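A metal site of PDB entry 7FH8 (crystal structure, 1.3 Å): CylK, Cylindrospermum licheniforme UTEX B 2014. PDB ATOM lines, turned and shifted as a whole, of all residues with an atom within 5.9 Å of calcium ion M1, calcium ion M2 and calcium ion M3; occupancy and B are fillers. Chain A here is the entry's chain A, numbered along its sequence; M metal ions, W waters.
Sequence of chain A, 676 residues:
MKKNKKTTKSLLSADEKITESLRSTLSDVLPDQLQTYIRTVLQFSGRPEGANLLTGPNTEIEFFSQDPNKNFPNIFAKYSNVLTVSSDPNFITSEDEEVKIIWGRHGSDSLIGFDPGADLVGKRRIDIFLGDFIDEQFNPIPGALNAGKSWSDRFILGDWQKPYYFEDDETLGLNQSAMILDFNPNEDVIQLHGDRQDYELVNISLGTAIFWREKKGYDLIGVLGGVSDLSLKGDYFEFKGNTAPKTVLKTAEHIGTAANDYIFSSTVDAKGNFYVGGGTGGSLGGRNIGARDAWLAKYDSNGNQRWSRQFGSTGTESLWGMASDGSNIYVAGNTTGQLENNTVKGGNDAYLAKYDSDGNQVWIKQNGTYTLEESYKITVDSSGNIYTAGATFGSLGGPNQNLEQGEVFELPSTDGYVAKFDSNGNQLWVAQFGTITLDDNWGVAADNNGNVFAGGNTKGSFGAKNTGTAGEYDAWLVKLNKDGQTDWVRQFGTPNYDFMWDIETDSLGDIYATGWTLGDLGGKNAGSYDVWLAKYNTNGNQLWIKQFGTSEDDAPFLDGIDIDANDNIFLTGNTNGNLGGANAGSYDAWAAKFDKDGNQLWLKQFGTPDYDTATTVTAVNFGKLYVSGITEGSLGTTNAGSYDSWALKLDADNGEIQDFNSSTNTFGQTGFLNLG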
ATOM      1  N   LEU A  83      -0.186  13.958  11.502  1.00  0.00           N
ATOM      2  CA  LEU A  83      -0.328  12.965  10.453  1.00  0.00           C
ATOM      3  C   LEU A  83      -1.207  13.516   9.327  1.00  0.00           C
ATOM      4  O   LEU A  83      -1.438  14.726   9.243  1.00  0.00           O
ATOM      5  CB  LEU A  83      -0.753  11.622  11.057  1.00  0.00           C
ATOM      6  CG  LEU A  83       0.325  11.065  11.977  1.00  0.00           C
ATOM      7  CD1 LEU A  83      -0.200   9.889  12.755  1.00  0.00           C
ATOM      8  CD2 LEU A  83       1.540  10.648  11.167  1.00  0.00           C
ATOM      9  N   THR A  84      -1.694  12.654   8.430  1.00  0.00           N
ATOM     10  CA  THR A  84      -2.307  13.107   7.182  1.00  0.00           C
ATOM     11  C   THR A  84      -3.812  12.875   7.195  1.00  0.00           C
ATOM     12  O   THR A  84      -4.383  12.340   8.153  1.00  0.00           O
ATOM     13  CB  THR A  84      -1.677  12.439   5.947  1.00  0.00           C
ATOM     14  OG1 THR A  84      -2.233  11.126   5.734  1.00  0.00           O
ATOM     15  CG2 THR A  84      -0.151  12.351   6.063  1.00  0.00           C
ATOM     16  N   VAL A  85      -4.456  13.262   6.092  1.00  0.00           N
ATOM     17  CA  VAL A  85      -5.877  12.978   5.906  1.00  0.00           C
ATOM     18  C   VAL A  85      -6.128  11.501   5.616  1.00  0.00           C
ATOM     19  O   VAL A  85      -7.277  11.064   5.620  1.00  0.00           O
ATOM     20  CB  VAL A  85      -6.440  13.962   4.856  1.00  0.00           C
ATOM     21  CG1 VAL A  85      -7.945  13.815   4.702  1.00  0.00           C
ATOM     22  CG2 VAL A  85      -6.097  15.400   5.217  1.00  0.00           C
ATOM     23  N   SER A  86      -5.073  10.728   5.372  1.00  0.00           N
ATOM     24  CA  SER A  86      -5.152   9.300   5.107  1.00  0.00           C
ATOM     25  C   SER A  86      -5.329   8.520   6.398  1.00  0.00           C
ATOM     26  O   SER A  86      -5.174   9.045   7.506  1.00  0.00           O
ATOM     27  CB  SER A  86      -3.846   8.793   4.485  1.00  0.00           C
ATOM     28  OG  SER A  86      -3.319   9.729   3.557  1.00  0.00           O
ATOM     29  N   SER A  87      -5.613   7.219   6.259  1.00  0.00           N
ATOM     30  CA  SER A  87      -5.557   6.304   7.395  1.00  0.00           C
ATOM     31  C   SER A  87      -4.091   5.943   7.619  1.00  0.00           C
ATOM     32  O   SER A  87      -3.512   5.144   6.884  1.00  0.00           O
ATOM     33  CB  SER A  87      -6.400   5.066   7.116  1.00  0.00           C
ATOM     34  OG  SER A  87      -7.750   5.456   6.955  1.00  0.00           O
ATOM     35  N   ASP A  88      -3.481   6.570   8.636  1.00  0.00           N
ATOM     36  CA  ASP A  88      -2.024   6.568   8.786  1.00  0.00           C
ATOM     37  C   ASP A  88      -1.566   5.610   9.877  1.00  0.00           C
ATOM     38  O   ASP A  88      -2.085   5.643  10.997  1.00  0.00           O
ATOM     39  CB  ASP A  88      -1.541   7.953   9.252  1.00  0.00           C
ATOM     40  CG  ASP A  88      -1.906   9.072   8.309  1.00  0.00           C
ATOM     41  OD1 ASP A  88      -1.441   9.042   7.143  1.00  0.00           O
ATOM     42  OD2 ASP A  88      -2.621   9.999   8.738  1.00  0.00           O
ATOM     43  N   TRP A 103      -1.294  13.534  16.335  1.00  0.00           N
ATOM     44  CA  TRP A 103      -2.574  14.010  15.818  1.00  0.00           C
ATOM     45  C   TRP A 103      -2.900  13.242  14.534  1.00  0.00           C
ATOM     46  O   TRP A 103      -2.303  13.471  13.487  1.00  0.00           O
ATOM     47  CB  TRP A 103      -2.494  15.511  15.578  1.00  0.00           C
ATOM     48  CG  TRP A 103      -3.762  16.158  15.136  1.00  0.00           C
ATOM     49  CD1 TRP A 103      -5.033  15.677  15.283  1.00  0.00           C
ATOM     50  CD2 TRP A 103      -3.890  17.409  14.464  1.00  0.00           C
ATOM     51  NE1 TRP A 103      -5.945  16.564  14.754  1.00  0.00           N
ATOM     52  CE2 TRP A 103      -5.263  17.639  14.255  1.00  0.00           C
ATOM     53  CE3 TRP A 103      -2.965  18.370  14.021  1.00  0.00           C
ATOM     54  CZ2 TRP A 103      -5.735  18.775  13.601  1.00  0.00           C
ATOM     55  CZ3 TRP A 103      -3.446  19.488  13.371  1.00  0.00           C
ATOM     56  CH2 TRP A 103      -4.817  19.685  13.169  1.00  0.00           C
ATOM     57  N   GLY A 104      -3.884  12.328  14.627  1.00  0.00           N
ATOM     58  CA  GLY A 104      -4.189  11.471  13.488  1.00  0.00           C
ATOM     59  C   GLY A 104      -4.932  12.160  12.359  1.00  0.00           C
ATOM     60  O   GLY A 104      -4.756  11.802  11.188  1.00  0.00           O
ATOM     61  N   ARG A 105      -5.770  13.143  12.680  1.00  0.00           N
ATOM     62  CA  ARG A 105      -6.642  13.789  11.687  1.00  0.00           C
ATOM     63  C   ARG A 105      -7.563  12.753  11.045  1.00  0.00           C
ATOM     64  O   ARG A 105      -7.891  11.729  11.660  1.00  0.00           O
ATOM     65  CB  ARG A 105      -5.858  14.688  10.735  1.00  0.00           C
ATOM     66  CG  ARG A 105      -5.196  15.854  11.456  1.00  0.00           C
ATOM     67  CD  ARG A 105      -4.200  16.590  10.579  1.00  0.00           C
ATOM     68  NE  ARG A 105      -4.796  17.276   9.444  1.00  0.00           N
ATOM     69  CZ  ARG A 105      -4.289  17.302   8.220  1.00  0.00           C
ATOM     70  NH1 ARG A 105      -3.181  16.638   7.921  1.00  0.00           N
ATOM     71  NH2 ARG A 105      -4.891  18.036   7.278  1.00  0.00           N
ATOM     72  N   HIS A 106      -8.000  13.000   9.812  1.00  0.00           N
ATOM     73  CA  HIS A 106      -8.968  12.126   9.187  1.00  0.00           C
ATOM     74  C   HIS A 106      -8.376  10.742   8.973  1.00  0.00           C
ATOM     75  O   HIS A 106      -7.159  10.534   9.012  1.00  0.00           O
ATOM     76  CB  HIS A 106      -9.388  12.674   7.823  1.00  0.00           C
ATOM     77  CG  HIS A 106      -9.623  14.153   7.812  1.00  0.00           C
ATOM     78  ND1 HIS A 106      -8.602  15.061   8.013  1.00  0.00           N
ATOM     79  CD2 HIS A 106     -10.741  14.884   7.600  1.00  0.00           C
ATOM     80  CE1 HIS A 106      -9.092  16.284   7.938  1.00  0.00           C
ATOM     81  NE2 HIS A 106     -10.384  16.205   7.685  1.00  0.00           N
ATOM     82  N   GLY A 107      -9.260   9.778   8.719  1.00  0.00           N
ATOM     83  CA  GLY A 107      -8.836   8.419   8.465  1.00  0.00           C
ATOM     84  C   GLY A 107      -8.759   7.581   9.729  1.00  0.00           C
ATOM     85  O   GLY A 107      -8.785   8.071  10.853  1.00  0.00           O
ATOM     86  N   SER A 108      -8.661   6.261   9.513  1.00  0.00           N
ATOM     87  CA  SER A 108      -8.607   5.277  10.590  1.00  0.00           C
ATOM     88  C   SER A 108      -7.133   5.063  10.930  1.00  0.00           C
ATOM     89  O   SER A 108      -6.438   4.259  10.308  1.00  0.00           O
ATOM     90  CB  SER A 108      -9.239   3.974  10.123  1.00  0.00           C
ATOM     91  OG  SER A 108     -10.577   4.195   9.703  1.00  0.00           O
ATOM     92  N   ASP A 109      -6.641   5.804  11.907  1.00  0.00           N
ATOM     93  CA  ASP A 109      -5.210   5.862  12.157  1.00  0.00           C
ATOM     94  C   ASP A 109      -4.765   4.811  13.166  1.00  0.00           C
ATOM     95  O   ASP A 109      -5.494   4.471  14.102  1.00  0.00           O
ATOM     96  CB  ASP A 109      -4.802   7.253  12.644  1.00  0.00           C
ATOM     97  CG  ASP A 109      -5.215   8.338  11.654  1.00  0.00           C
ATOM     98  OD1 ASP A 109      -4.700   8.313  10.512  1.00  0.00           O
ATOM     99  OD2 ASP A 109      -6.070   9.185  11.988  1.00  0.00           O
ATOM    100  N   LEU A 130      -4.561  12.475  19.730  1.00  0.00           N
ATOM    101  CA  LEU A 130      -5.839  12.891  19.152  1.00  0.00           C
ATOM    102  C   LEU A 130      -6.094  11.975  17.961  1.00  0.00           C
ATOM    103  O   LEU A 130      -5.420  12.070  16.932  1.00  0.00           O
ATOM    104  CB  LEU A 130      -5.784  14.358  18.711  1.00  0.00           C
ATOM    105  CG  LEU A 130      -5.626  15.384  19.839  1.00  0.00           C
ATOM    106  CD1 LEU A 130      -5.025  16.667  19.287  1.00  0.00           C
ATOM    107  CD2 LEU A 130      -6.985  15.665  20.458  1.00  0.00           C
ATOM    108  N   GLY A 131      -7.067  11.067  18.103  1.00  0.00           N
ATOM    109  CA  GLY A 131      -7.333  10.126  17.019  1.00  0.00           C
ATOM    110  C   GLY A 131      -7.848  10.803  15.770  1.00  0.00           C
ATOM    111  O   GLY A 131      -7.431  10.490  14.654  1.00  0.00           O
ATOM    112  N   ASP A 132      -8.796  11.736  15.944  1.00  0.00           N
ATOM    113  CA  ASP A 132      -9.357  12.478  14.832  1.00  0.00           C
ATOM    114  C   ASP A 132      -9.102  13.965  15.033  1.00  0.00           C
ATOM    115  O   ASP A 132      -8.067  14.465  14.579  1.00  0.00           O
ATOM    116  CB  ASP A 132     -10.852  12.154  14.667  1.00  0.00           C
ATOM    117  CG  ASP A 132     -11.085  10.768  14.076  1.00  0.00           C
ATOM    118  OD1 ASP A 132     -10.365  10.384  13.126  1.00  0.00           O
ATOM    119  OD2 ASP A 132     -11.985  10.043  14.566  1.00  0.00           O
ATOM    120  N   ILE A 134     -10.535  16.545  13.620  1.00  0.00           N
ATOM    121  CA  ILE A 134     -10.244  16.874  12.229  1.00  0.00           C
ATOM    122  C   ILE A 134     -10.314  18.374  11.967  1.00  0.00           C
ATOM    123  O   ILE A 134     -10.904  19.148  12.723  1.00  0.00           O
ATOM    124  CB  ILE A 134     -11.129  16.081  11.249  1.00  0.00           C
ATOM    125  CG1 ILE A 134     -12.591  16.531  11.362  1.00  0.00           C
ATOM    126  CG2 ILE A 134     -10.940  14.569  11.459  1.00  0.00           C
ATOM    127  CD1 ILE A 134     -13.507  15.868  10.345  1.00  0.00           C
ATOM    128  N   SER A 150     -16.069  11.054  11.794  1.00  0.00           N
ATOM    129  CA  SER A 150     -14.967  10.513  12.594  1.00  0.00           C
ATOM    130  C   SER A 150     -14.680   9.100  12.117  1.00  0.00           C
ATOM    131  O   SER A 150     -15.449   8.515  11.347  1.00  0.00           O
ATOM    132  CB  SER A 150     -15.282  10.560  14.089  1.00  0.00           C
ATOM    133  OG  SER A 150     -16.476   9.860  14.378  1.00  0.00           O
ATOM    134  N   TRP A 151     -13.560   8.553  12.591  1.00  0.00           N
ATOM    135  CA  TRP A 151     -13.063   7.267  12.121  1.00  0.00           C
ATOM    136  C   TRP A 151     -12.652   6.424  13.318  1.00  0.00           C
ATOM    137  O   TRP A 151     -12.396   6.930  14.405  1.00  0.00           O
ATOM    138  CB  TRP A 151     -11.841   7.458  11.210  1.00  0.00           C
ATOM    139  CG  TRP A 151     -12.183   7.940   9.821  1.00  0.00           C
ATOM    140  CD1 TRP A 151     -12.324   7.179   8.699  1.00  0.00           C
ATOM    141  CD2 TRP A 151     -12.453   9.300   9.424  1.00  0.00           C
ATOM    142  NE1 TRP A 151     -12.654   7.979   7.626  1.00  0.00           N
ATOM    143  CE2 TRP A 151     -12.746   9.276   8.047  1.00  0.00           C
ATOM    144  CE3 TRP A 151     -12.467  10.528  10.097  1.00  0.00           C
ATOM    145  CZ2 TRP A 151     -13.053  10.431   7.331  1.00  0.00           C
ATOM    146  CZ3 TRP A 151     -12.788  11.670   9.392  1.00  0.00           C
ATOM    147  CH2 TRP A 151     -13.071  11.618   8.012  1.00  0.00           C
ATOM    148  N   SER A 152     -12.566   5.111  13.102  1.00  0.00           N
ATOM    149  CA  SER A 152     -12.022   4.203  14.103  1.00  0.00           C
ATOM    150  C   SER A 152     -10.507   4.341  14.142  1.00  0.00           C
ATOM    151  O   SER A 152      -9.816   3.928  13.200  1.00  0.00           O
ATOM    152  CB  SER A 152     -12.417   2.770  13.754  1.00  0.00           C
ATOM    153  OG  SER A 152     -13.818   2.593  13.776  1.00  0.00           O
ATOM    154  N   ASP A 153      -9.973   4.905  15.221  1.00  0.00           N
ATOM    155  CA  ASP A 153      -8.548   5.000  15.428  1.00  0.00           C
ATOM    156  C   ASP A 153      -8.132   3.972  16.472  1.00  0.00           C
ATOM    157  O   ASP A 153      -8.903   3.658  17.385  1.00  0.00           O
ATOM    158  CB  ASP A 153      -8.148   6.394  15.908  1.00  0.00           C
ATOM    159  CG  ASP A 153      -8.644   7.466  14.986  1.00  0.00           C
ATOM    160  OD1 ASP A 153      -8.133   7.533  13.841  1.00  0.00           O
ATOM    161  OD2 ASP A 153      -9.544   8.235  15.375  1.00  0.00           O
ATOM    162  N   PHE A 155      -5.344   3.265  19.309  1.00  0.00           N
ATOM    163  CA  PHE A 155      -4.351   3.908  20.156  1.00  0.00           C
ATOM    164  C   PHE A 155      -3.499   2.795  20.761  1.00  0.00           C
ATOM    165  O   PHE A 155      -4.000   1.984  21.548  1.00  0.00           O
ATOM    166  CB  PHE A 155      -5.003   4.746  21.252  1.00  0.00           C
ATOM    167  CG  PHE A 155      -5.916   5.827  20.731  1.00  0.00           C
ATOM    168  CD1 PHE A 155      -5.396   7.054  20.305  1.00  0.00           C
ATOM    169  CD2 PHE A 155      -7.289   5.642  20.680  1.00  0.00           C
ATOM    170  CE1 PHE A 155      -6.230   8.055  19.842  1.00  0.00           C
ATOM    171  CE2 PHE A 155      -8.136   6.649  20.216  1.00  0.00           C
ATOM    172  CZ  PHE A 155      -7.600   7.859  19.800  1.00  0.00           C
ATOM    173  N   ASP A 182      -9.520  12.242  22.827  1.00  0.00           N
ATOM    174  CA  ASP A 182     -10.771  12.141  22.077  1.00  0.00           C
ATOM    175  C   ASP A 182     -11.169  10.685  21.869  1.00  0.00           C
ATOM    176  O   ASP A 182     -11.712  10.314  20.820  1.00  0.00           O
ATOM    177  CB  ASP A 182     -10.686  12.861  20.733  1.00  0.00           C
ATOM    178  CG  ASP A 182      -9.777  12.151  19.740  1.00  0.00           C
ATOM    179  OD1 ASP A 182      -8.793  11.531  20.203  1.00  0.00           O
ATOM    180  OD2 ASP A 182     -10.048  12.186  18.516  1.00  0.00           O
ATOM    181  N   ASN A 184     -13.332   7.664  21.634  1.00  0.00           N
ATOM    182  CA  ASN A 184     -14.760   7.413  21.478  1.00  0.00           C
ATOM    183  C   ASN A 184     -14.972   5.899  21.545  1.00  0.00           C
ATOM    184  O   ASN A 184     -14.620   5.202  20.588  1.00  0.00           O
ATOM    185  CB  ASN A 184     -15.248   7.965  20.141  1.00  0.00           C
ATOM    186  CG  ASN A 184     -16.735   7.726  19.916  1.00  0.00           C
ATOM    187  OD1 ASN A 184     -17.369   6.946  20.615  1.00  0.00           O
ATOM    188  ND2 ASN A 184     -17.302   8.420  18.928  1.00  0.00           N
ATOM    189  N   GLU A 187     -16.259   3.760  18.544  1.00  0.00           N
ATOM    190  CA  GLU A 187     -15.537   3.630  17.279  1.00  0.00           C
ATOM    191  C   GLU A 187     -14.069   3.239  17.480  1.00  0.00           C
ATOM    192  O   GLU A 187     -13.541   2.434  16.707  1.00  0.00           O
ATOM    193  CB  GLU A 187     -15.628   4.928  16.450  1.00  0.00           C
ATOM    194  CG  GLU A 187     -14.977   6.154  17.110  1.00  0.00           C
ATOM    195  CD  GLU A 187     -14.961   7.413  16.235  1.00  0.00           C
ATOM    196  OE1 GLU A 187     -15.852   7.542  15.363  1.00  0.00           O
ATOM    197  OE2 GLU A 187     -14.064   8.274  16.421  1.00  0.00           O
ATOM    198  N   ASP A 188     -13.402   3.822  18.470  1.00  0.00           N
ATOM    199  CA  ASP A 188     -11.961   3.688  18.603  1.00  0.00           C
ATOM    200  C   ASP A 188     -11.589   2.423  19.370  1.00  0.00           C
ATOM    201  O   ASP A 188     -12.436   1.789  20.019  1.00  0.00           O
ATOM    202  CB  ASP A 188     -11.373   4.897  19.353  1.00  0.00           C
ATOM    203  CG  ASP A 188     -11.543   6.207  18.608  1.00  0.00           C
ATOM    204  OD1 ASP A 188     -11.483   6.250  17.366  1.00  0.00           O
ATOM    205  OD2 ASP A 188     -11.730   7.237  19.292  1.00  0.00           O
HETATM  206 CA    CA M   1      -4.867  10.374   9.358  1.00  0.00          CA
HETATM  207 CA    CA M   2      -8.233   9.571  12.628  1.00  0.00          CA
HETATM  208 CA    CA M   3     -11.730   8.277  16.096  1.00  0.00          CA
HETATM  209  O   HOH W   1     -11.085   9.559  17.954  1.00  0.00           O
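The side-chain hydroxyl (OG) of Ser 86 lies within hydrogen-bond range of the side-chain hydroxyl (OG1) of Thr 84, at 2.8 Å. The backbone NH (N) of Gly 104 is in hydrogen-bond range of the backbone carbonyl oxygen (O) of Leu 130 (2.8 Å). N of Asp 132 lies within hydrogen-bond range of OD2 of Asp 182, at 2.9 Å. The indole nitrogen of Trp 103 lies within hydrogen-bond range of the backbone carbonyl oxygen of Asp 132. OE1 of Glu 187 sits at hydrogen-bond distance from OG of Ser 150 (2.6 Å). The backbone NH (N) of Gly 131 lies within hydrogen-bond range of the side-chain carboxylate (OD1) of Asp 182 (2.8 Å). The guanidinium group of Arg 105 is in hydrogen-bond range of the backbone carbonyl oxygen of Leu 83 (2.9 Å). The side-chain carboxylate (OD2) of Asp 188 sits at hydrogen-bond distance from the backbone NH (N) of Asn 184 (2.9 Å).
Within 4 Å of calcium ion M2: Arg 105, His 106, Gly 107, Asp 109, Gly 131, Asp 132 and Asp 153. The nearest printed residue that does not touch calcium ion M2 is Gly 104 (4.2 Å).
Within 4 Å of calcium ion M3: Asp 132, Trp 151, Asp 153, Glu 187 and Asp 188.
Calcium ion M1 is bound by the backbone carbonyl oxygen (O) of Ser 86 (2.3 Å), the backbone carbonyl oxygen (O) of His 106 (2.3 Å), the backbone carbonyl oxygen (O) of Gly 104 (2.3 Å), the backbone carbonyl oxygen (O) of Thr 84 (2.4 Å), the side-chain carboxylate (OD2) of Asp 88 (2.4 Å) and the side-chain carboxylate (OD1) of Asp 109 (2.4 Å). Slightly farther from calcium ion M1 lies OD2 of Asp 109 (3.1 Å).
Calcium ion M2 is bound by OD2 of Asp 109 (2.3 Å), OD1 of Asp 132 (2.3 Å), O of Gly 131 (2.4 Å), OD1 of Asp 153 (2.4 Å), O of Gly 107 (2.4 Å) and O of Arg 105 (2.4 Å). Calcium ion M2 has six donor atoms within binding distance.
Calcium ion M3 is bound by the backbone carbonyl oxygen of Trp 151 (2.3 Å), the side-chain carboxylate of Asp 153 (2.3 Å), water W1 (2.3 Å), the side-chain carboxylate of Asp 132 (2.4 Å), the side-chain carboxylate of Glu 187 (2.4 Å) and the side-chain carboxylate of Asp 188 (2.4 Å). Calcium ion M3 has six donor atoms within binding distance.
Water W1 lies within hydrogen-bond range of OD2 of Asp 188 and OD2 of Asp 182.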
